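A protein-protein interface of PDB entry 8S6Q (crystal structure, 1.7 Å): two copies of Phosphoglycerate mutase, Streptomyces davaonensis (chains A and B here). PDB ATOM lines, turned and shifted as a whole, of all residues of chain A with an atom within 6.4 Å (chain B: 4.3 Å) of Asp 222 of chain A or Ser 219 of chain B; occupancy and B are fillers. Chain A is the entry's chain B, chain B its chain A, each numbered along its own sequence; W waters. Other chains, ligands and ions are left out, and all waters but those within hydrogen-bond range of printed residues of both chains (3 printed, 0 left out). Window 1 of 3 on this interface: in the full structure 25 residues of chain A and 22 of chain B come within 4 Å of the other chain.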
ATOM      1  N   LEU A  76     -36.808  13.737  13.782  1.00  0.00           N
ATOM      2  CA  LEU A  76     -37.020  15.128  13.412  1.00  0.00           C
ATOM      3  C   LEU A  76     -37.975  15.809  14.382  1.00  0.00           C
ATOM      4  O   LEU A  76     -37.702  16.913  14.864  1.00  0.00           O
ATOM      5  CB  LEU A  76     -37.557  15.210  11.965  1.00  0.00           C
ATOM      6  CG  LEU A  76     -37.972  16.592  11.474  1.00  0.00           C
ATOM      7  CD1 LEU A  76     -36.676  17.378  11.168  1.00  0.00           C
ATOM      8  CD2 LEU A  76     -38.914  16.472  10.251  1.00  0.00           C
ATOM      9  N   ARG A  79     -36.221  16.486  17.503  1.00  0.00           N
ATOM     10  CA  ARG A  79     -35.286  17.606  17.365  1.00  0.00           C
ATOM     11  C   ARG A  79     -36.019  18.944  17.406  1.00  0.00           C
ATOM     12  O   ARG A  79     -35.574  19.889  18.062  1.00  0.00           O
ATOM     13  CB  ARG A  79     -34.489  17.469  16.070  1.00  0.00           C
ATOM     14  CG  ARG A  79     -33.788  18.739  15.656  1.00  0.00           C
ATOM     15  CD  ARG A  79     -33.312  18.570  14.203  1.00  0.00           C
ATOM     16  NE  ARG A  79     -32.428  19.678  13.840  1.00  0.00           N
ATOM     17  CZ  ARG A  79     -31.691  19.760  12.736  1.00  0.00           C
ATOM     18  NH1 ARG A  79     -31.617  18.767  11.869  1.00  0.00           N
ATOM     19  NH2 ARG A  79     -30.941  20.837  12.546  1.00  0.00           N
ATOM     20  N   MET A 198     -26.067  19.535  -4.522  1.00  0.00           N
ATOM     21  CA  MET A 198     -26.375  18.766  -3.321  1.00  0.00           C
ATOM     22  C   MET A 198     -27.730  18.060  -3.428  1.00  0.00           C
ATOM     23  O   MET A 198     -28.654  18.550  -4.095  1.00  0.00           O
ATOM     24  CB  MET A 198     -26.400  19.625  -2.052  1.00  0.00           C
ATOM     25  CG  MET A 198     -25.143  20.384  -1.559  1.00  0.00           C
ATOM     26  SD  MET A 198     -25.745  21.843  -0.652  1.00  0.00           S
ATOM     27  CE  MET A 198     -25.624  21.073   1.022  1.00  0.00           C
ATOM     28  N   LEU A 200     -30.741  16.944  -0.797  1.00  0.00           N
ATOM     29  CA  LEU A 200     -31.181  17.150   0.574  1.00  0.00           C
ATOM     30  C   LEU A 200     -31.549  15.797   1.175  1.00  0.00           C
ATOM     31  O   LEU A 200     -32.334  15.053   0.572  1.00  0.00           O
ATOM     32  CB  LEU A 200     -32.373  18.088   0.615  1.00  0.00           C
ATOM     33  CG  LEU A 200     -32.136  19.479   0.001  1.00  0.00           C
ATOM     34  CD1 LEU A 200     -33.479  20.247  -0.071  1.00  0.00           C
ATOM     35  CD2 LEU A 200     -31.040  20.301   0.760  1.00  0.00           C
ATOM     36  N   PRO A 201     -30.964  15.422   2.297  1.00  0.00           N
ATOM     37  CA  PRO A 201     -31.383  14.193   2.977  1.00  0.00           C
ATOM     38  C   PRO A 201     -32.854  14.232   3.338  1.00  0.00           C
ATOM     39  O   PRO A 201     -33.439  15.294   3.557  1.00  0.00           O
ATOM     40  CB  PRO A 201     -30.524  14.167   4.242  1.00  0.00           C
ATOM     41  CG  PRO A 201     -29.318  15.063   3.946  1.00  0.00           C
ATOM     42  CD  PRO A 201     -29.874  16.137   2.990  1.00  0.00           C
ATOM     43  N   THR A 203     -35.861  14.269   5.683  1.00  0.00           N
ATOM     44  CA  THR A 203     -36.066  15.012   6.937  1.00  0.00           C
ATOM     45  C   THR A 203     -34.970  16.047   7.200  1.00  0.00           C
ATOM     46  O   THR A 203     -34.837  16.529   8.344  1.00  0.00           O
ATOM     47  CB  THR A 203     -36.241  14.115   8.197  1.00  0.00           C
ATOM     48  OG1 THR A 203     -35.037  13.433   8.554  1.00  0.00           O
ATOM     49  CG2 THR A 203     -37.398  13.097   8.053  1.00  0.00           C
ATOM     50  N   SER A 204     -34.193  16.458   6.187  1.00  0.00           N
ATOM     51  CA  SER A 204     -33.222  17.496   6.467  1.00  0.00           C
ATOM     52  C   SER A 204     -33.945  18.831   6.628  1.00  0.00           C
ATOM     53  O   SER A 204     -35.061  19.048   6.125  1.00  0.00           O
ATOM     54  CB  SER A 204     -32.160  17.590   5.350  1.00  0.00           C
ATOM     55  OG  SER A 204     -32.768  18.040   4.139  1.00  0.00           O
ATOM     56  N   VAL A 205     -33.288  19.699   7.384  1.00  0.00           N
ATOM     57  CA  VAL A 205     -33.740  21.036   7.731  1.00  0.00           C
ATOM     58  C   VAL A 205     -32.818  22.000   7.016  1.00  0.00           C
ATOM     59  O   VAL A 205     -31.581  21.893   7.129  1.00  0.00           O
ATOM     60  CB  VAL A 205     -33.650  21.274   9.250  1.00  0.00           C
ATOM     61  CG1 VAL A 205     -33.850  22.723   9.607  1.00  0.00           C
ATOM     62  CG2 VAL A 205     -34.671  20.377   9.967  1.00  0.00           C
ATOM     63  N   SER A 206     -33.414  22.922   6.274  1.00  0.00           N
ATOM     64  CA  SER A 206     -32.708  24.053   5.670  1.00  0.00           C
ATOM     65  C   SER A 206     -33.401  25.341   6.105  1.00  0.00           C
ATOM     66  O   SER A 206     -34.612  25.476   5.909  1.00  0.00           O
ATOM     67  CB  SER A 206     -32.766  23.944   4.142  1.00  0.00           C
ATOM     68  OG  SER A 206     -32.286  22.701   3.675  1.00  0.00           O
ATOM     69  N   SER A 219     -28.996  28.074   6.059  1.00  0.00           N
ATOM     70  CA  SER A 219     -28.357  26.768   6.204  1.00  0.00           C
ATOM     71  C   SER A 219     -29.054  25.797   5.265  1.00  0.00           C
ATOM     72  O   SER A 219     -30.214  26.002   4.888  1.00  0.00           O
ATOM     73  CB  SER A 219     -28.421  26.217   7.647  1.00  0.00           C
ATOM     74  OG  SER A 219     -29.763  26.233   8.101  1.00  0.00           O
ATOM     75  N   ILE A 220     -28.344  24.718   4.896  1.00  0.00           N
ATOM     76  CA  ILE A 220     -28.821  23.801   3.861  1.00  0.00           C
ATOM     77  C   ILE A 220     -28.594  22.356   4.281  1.00  0.00           C
ATOM     78  O   ILE A 220     -27.448  21.951   4.493  1.00  0.00           O
ATOM     79  CB  ILE A 220     -28.117  23.997   2.510  1.00  0.00           C
ATOM     80  CG1 ILE A 220     -28.137  25.444   2.087  1.00  0.00           C
ATOM     81  CG2 ILE A 220     -28.896  23.153   1.520  1.00  0.00           C
ATOM     82  CD1 ILE A 220     -27.477  25.616   0.715  1.00  0.00           C
ATOM     83  N   GLY A 221     -29.666  21.557   4.282  1.00  0.00           N
ATOM     84  CA  GLY A 221     -29.535  20.117   4.169  1.00  0.00           C
ATOM     85  C   GLY A 221     -29.165  19.381   5.446  1.00  0.00           C
ATOM     86  O   GLY A 221     -28.641  18.252   5.382  1.00  0.00           O
ATOM     87  N   ASP A 222     -29.419  19.971   6.606  1.00  0.00           N
ATOM     88  CA  ASP A 222     -28.936  19.357   7.845  1.00  0.00           C
ATOM     89  C   ASP A 222     -29.864  18.230   8.295  1.00  0.00           C
ATOM     90  O   ASP A 222     -31.035  18.470   8.591  1.00  0.00           O
ATOM     91  CB  ASP A 222     -28.814  20.384   8.962  1.00  0.00           C
ATOM     92  CG  ASP A 222     -28.240  19.790  10.219  1.00  0.00           C
ATOM     93  OD1 ASP A 222     -28.934  19.002  10.879  1.00  0.00           O
ATOM     94  OD2 ASP A 222     -27.097  20.130  10.556  1.00  0.00           O
ATOM     95  N   ALA A 223     -29.327  17.017   8.358  1.00  0.00           N
ATOM     96  CA  ALA A 223     -30.063  15.863   8.848  1.00  0.00           C
ATOM     97  C   ALA A 223     -29.334  15.241  10.029  1.00  0.00           C
ATOM     98  O   ALA A 223     -29.387  14.044  10.207  1.00  0.00           O
ATOM     99  CB  ALA A 223     -30.246  14.843   7.729  1.00  0.00           C
ATOM    100  N   THR A 224     -28.599  16.044  10.798  1.00  0.00           N
ATOM    101  CA  THR A 224     -27.758  15.512  11.864  1.00  0.00           C
ATOM    102  C   THR A 224     -28.560  14.776  12.935  1.00  0.00           C
ATOM    103  O   THR A 224     -27.961  14.019  13.698  1.00  0.00           O
ATOM    104  CB  THR A 224     -26.935  16.628  12.505  1.00  0.00           C
ATOM    105  OG1 THR A 224     -27.812  17.661  12.950  1.00  0.00           O
ATOM    106  CG2 THR A 224     -25.923  17.219  11.487  1.00  0.00           C
ATOM    107  N   HIS A 225     -29.883  14.948  12.994  1.00  0.00           N
ATOM    108  CA  HIS A 225     -30.678  14.203  13.983  1.00  0.00           C
ATOM    109  C   HIS A 225     -30.775  12.722  13.647  1.00  0.00           C
ATOM    110  O   HIS A 225     -31.129  11.922  14.511  1.00  0.00           O
ATOM    111  CB  HIS A 225     -32.051  14.849  14.070  1.00  0.00           C
ATOM    112  CG  HIS A 225     -32.725  14.917  12.719  1.00  0.00           C
ATOM    113  ND1 HIS A 225     -32.641  16.038  11.916  1.00  0.00           N
ATOM    114  CD2 HIS A 225     -33.482  14.019  12.045  1.00  0.00           C
ATOM    115  CE1 HIS A 225     -33.301  15.818  10.792  1.00  0.00           C
ATOM    116  NE2 HIS A 225     -33.845  14.611  10.849  1.00  0.00           N
ATOM    117  N   ARG B  79     -25.721  19.761  21.910  1.00  0.00           N
ATOM    118  CA  ARG B  79     -26.331  19.189  20.731  1.00  0.00           C
ATOM    119  C   ARG B  79     -25.483  18.004  20.278  1.00  0.00           C
ATOM    120  O   ARG B  79     -25.996  16.991  19.794  1.00  0.00           O
ATOM    121  CB  ARG B  79     -26.304  20.256  19.592  1.00  0.00           C
ATOM    122  CG  ARG B  79     -26.388  19.651  18.223  1.00  0.00           C
ATOM    123  CD  ARG B  79     -26.352  20.777  17.100  1.00  0.00           C
ATOM    124  NE  ARG B  79     -26.463  20.166  15.775  1.00  0.00           N
ATOM    125  CZ  ARG B  79     -26.541  20.853  14.636  1.00  0.00           C
ATOM    126  NH1 ARG B  79     -26.487  22.170  14.627  1.00  0.00           N
ATOM    127  NH2 ARG B  79     -26.751  20.201  13.495  1.00  0.00           N
ATOM    128  N   SER B 206     -21.426  22.161   9.555  1.00  0.00           N
ATOM    129  CA  SER B 206     -21.528  21.798   8.151  1.00  0.00           C
ATOM    130  C   SER B 206     -20.959  20.400   8.008  1.00  0.00           C
ATOM    131  O   SER B 206     -19.808  20.179   8.398  1.00  0.00           O
ATOM    132  CB  SER B 206     -20.708  22.783   7.293  1.00  0.00           C
ATOM    133  OG  SER B 206     -21.167  24.097   7.495  1.00  0.00           O
ATOM    134  N   VAL B 207     -21.701  19.474   7.415  1.00  0.00           N
ATOM    135  CA  VAL B 207     -21.244  18.096   7.343  1.00  0.00           C
ATOM    136  C   VAL B 207     -20.647  17.768   5.987  1.00  0.00           C
ATOM    137  O   VAL B 207     -21.264  18.059   4.938  1.00  0.00           O
ATOM    138  CB  VAL B 207     -22.394  17.143   7.672  1.00  0.00           C
ATOM    139  CG1 VAL B 207     -21.941  15.714   7.570  1.00  0.00           C
ATOM    140  CG2 VAL B 207     -22.920  17.487   9.050  1.00  0.00           C
ATOM    141  N   VAL B 217     -19.759  17.707   0.122  1.00  0.00           N
ATOM    142  CA  VAL B 217     -20.528  18.535   1.055  1.00  0.00           C
ATOM    143  C   VAL B 217     -21.927  17.958   1.214  1.00  0.00           C
ATOM    144  O   VAL B 217     -22.686  17.874   0.239  1.00  0.00           O
ATOM    145  CB  VAL B 217     -20.605  19.992   0.585  1.00  0.00           C
ATOM    146  CG1 VAL B 217     -21.553  20.805   1.508  1.00  0.00           C
ATOM    147  CG2 VAL B 217     -19.238  20.603   0.643  1.00  0.00           C
ATOM    148  N   ARG B 218     -22.288  17.630   2.458  1.00  0.00           N
ATOM    149  CA  ARG B 218     -23.635  17.140   2.727  1.00  0.00           C
ATOM    150  C   ARG B 218     -24.567  18.218   3.255  1.00  0.00           C
ATOM    151  O   ARG B 218     -25.733  18.235   2.891  1.00  0.00           O
ATOM    152  CB  ARG B 218     -23.585  15.988   3.729  1.00  0.00           C
ATOM    153  CG  ARG B 218     -22.974  14.707   3.217  1.00  0.00           C
ATOM    154  CD  ARG B 218     -24.074  13.717   2.762  1.00  0.00           C
ATOM    155  NE  ARG B 218     -23.590  12.342   2.796  1.00  0.00           N
ATOM    156  CZ  ARG B 218     -22.988  11.712   1.795  1.00  0.00           C
ATOM    157  NH1 ARG B 218     -22.849  12.272   0.601  1.00  0.00           N
ATOM    158  NH2 ARG B 218     -22.522  10.480   1.996  1.00  0.00           N
ATOM    159  N   SER B 219     -24.097  19.095   4.138  1.00  0.00           N
ATOM    160  CA  SER B 219     -24.950  20.163   4.650  1.00  0.00           C
ATOM    161  C   SER B 219     -24.064  21.344   5.030  1.00  0.00           C
ATOM    162  O   SER B 219     -22.859  21.193   5.213  1.00  0.00           O
ATOM    163  CB  SER B 219     -25.782  19.681   5.861  1.00  0.00           C
ATOM    164  OG  SER B 219     -24.875  19.251   6.862  1.00  0.00           O
ATOM    165  N   ILE B 220     -24.667  22.532   5.133  1.00  0.00           N
ATOM    166  CA  ILE B 220     -23.915  23.765   5.350  1.00  0.00           C
ATOM    167  C   ILE B 220     -24.613  24.680   6.348  1.00  0.00           C
ATOM    168  O   ILE B 220     -25.788  25.007   6.163  1.00  0.00           O
ATOM    169  CB  ILE B 220     -23.761  24.582   4.028  1.00  0.00           C
ATOM    170  CG1 ILE B 220     -23.316  23.678   2.888  1.00  0.00           C
ATOM    171  CG2 ILE B 220     -22.792  25.676   4.305  1.00  0.00           C
ATOM    172  CD1 ILE B 220     -23.228  24.413   1.473  1.00  0.00           C
ATOM    173  N   ASP B 222     -25.536  25.051   9.672  1.00  0.00           N
ATOM    174  CA  ASP B 222     -26.666  24.861  10.576  1.00  0.00           C
ATOM    175  C   ASP B 222     -26.317  25.342  11.984  1.00  0.00           C
ATOM    176  O   ASP B 222     -25.464  24.757  12.647  1.00  0.00           O
ATOM    177  CB  ASP B 222     -27.067  23.388  10.608  1.00  0.00           C
ATOM    178  CG  ASP B 222     -28.336  23.144  11.446  1.00  0.00           C
ATOM    179  OD1 ASP B 222     -28.239  23.335  12.688  1.00  0.00           O
ATOM    180  OD2 ASP B 222     -29.358  22.682  10.916  1.00  0.00           O
HETATM  181  O   HOH W   1     -29.902  23.495   8.306  1.00  0.00           O
HETATM  182  O   HOH W   2     -25.326  20.947   8.729  1.00  0.00           O
HETATM  183  O   HOH W   3     -26.334  16.852   7.580  1.00  0.00           O
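OD2 of Asp 222 of chain A is in salt-bridge range of NH2 of Arg 79 of chain B (3.0 Å). The side-chain hydroxyl (OG1) of Thr 224 of chain A lies within hydrogen-bond range of the guanidinium group (NH2) of Arg 79 of chain B. The backbone carbonyl oxygen (O) of Ile 220 of chain B is in hydrogen-bond range of the backbone NH (N) of Ile 220 of chain A (2.9 Å). The side-chain carboxylate of Asp 222 of chain B lies within salt-bridge range of the guanidinium group of Arg 79 of chain A, 2.9 Å away. The side-chain carboxylate (OD2) of Asp 222 of chain A sits close to the side-chain carboxylate (OD2) of Asp 222 of chain B (3.4 Å).
The side-chain carboxylate (OD1) of Asp 222 of chain B lies within salt-bridge range of the guanidinium group (NH1) of Arg 79 of chain B. O of Val 207 of chain B sits at hydrogen-bond distance from N of Arg 218 of chain B, at 2.7 Å. The guanidinium group (NH1) of Arg 79 of chain A lies within salt-bridge range of the side-chain carboxylate (OD1) of Asp 222 of chain A, 2.9 Å away. The backbone carbonyl oxygen (O) of Asp 222 of chain A lies within hydrogen-bond range of the backbone NH (N) of Val 205 of chain A, at 2.8 Å. N of Gly 221 of chain A sits at hydrogen-bond distance from OG of Ser 206 of chain A (2.9 Å). The side-chain hydroxyl (OG1) of Thr 224 of chain A sits at hydrogen-bond distance from the side-chain carboxylate (OD1) of Asp 222 of chain A (2.7 Å).
Met 198 of chain A touches Val 217 of chain B (CG to O, 3.9 Å). Met 198 of chain A touches Arg 218 of chain B (CE to O, 3.4 Å). Met 198 of chain A touches Ser 219 of chain B. Ile 220 of chain B touches Met 198 of chain A (CG1 to CE, 3.9 Å). Ser 219 of chain A touches Ile 220 of chain B. Ser 219 of chain A touches Asp 222 of chain B. Ile 220 of chain A touches Ser 219 of chain B. Arg 218 of chain B touches Gly 221 of chain A (O to O, 3.8 Å). O of Gly 221 of chain A touches CB of Ser 219 of chain B (3.2 Å). CB of Ser 219 of chain B touches N of Asp 222 of chain A (3.7 Å).
Ser 204 of chain A touches none of the printed residues of chain B. Of the printed residues of chain B, Ser 219 of chain A touches Ile 220 and Asp 222. Of chain B, only Arg 79, Ser 219 and Asp 222 come within 4 Å of Asp 222 of chain A. Printed residues of chain A within 4 Å of Arg 79 of chain B: Asp 222 (3.0 Å) and Thr 224 (2.8 Å). Of the printed residues of chain A, Val 207 of chain B touches Thr 224 (3.9 Å). Of chain A, only Met 198, Ile 220, Gly 221 and Asp 222 come within 4 Å of Ser 219 of chain B. Of the printed residues of chain A, Asp 222 of chain B touches Arg 79 (2.9 Å), Ser 219 (3.7 Å) and Asp 222 (3.1 Å). The nearest printed residue of chain B that does not touch Asp 222 of chain A is Val 207 of chain B (5.2 Å). The nearest residue of chain A that does not touch Ser 219 of chain B is Ala 223 of chain A (5.1 Å). The nearest printed residue of chain A that does not touch Val 207 of chain B is Asp 222 of chain A (5.2 Å).
Of the 16 printed residues of chain A, 7 touch a printed residue of chain B. Hydrophobic or aromatic side chains of chain B that line the printed part of chain A: Val 207 and Ile 220. Among the printed residues, 16 pairs touch across the chains.
Arg 79 of chain A touches Asp 222 of chain B, and with the chains exchanged Asp 222 of chain A touches Arg 79 of chain B. Ser 219 of chain A touches Asp 222 of chain B, and with the chains exchanged Asp 222 of chain A touches Ser 219 of chain B. Ile 220 of chain B touches its own counterpart, Ile 220 of chain A. Asp 222 of chain B touches its own counterpart, Asp 222 of chain A.
Water W2 lies within hydrogen-bond range of the side-chain hydroxyl of Ser 219 of chain B (2.6 Å) and the side-chain carboxylate of Asp 222 of chain A (2.7 Å). Water W1 lies within hydrogen-bond range of O of Val 205 of chain A (2.6 Å), OG of Ser 219 of chain A (2.7 Å) and OD2 of Asp 222 of chain B (2.8 Å). Water W3 lies within hydrogen-bond range of the side-chain hydroxyl (OG) of Ser 219 of chain B (2.9 Å), the backbone NH (N) of Ala 223 of chain A (3.1 Å) and the backbone carbonyl oxygen (O) of Gly 221 of chain A (3.5 Å).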
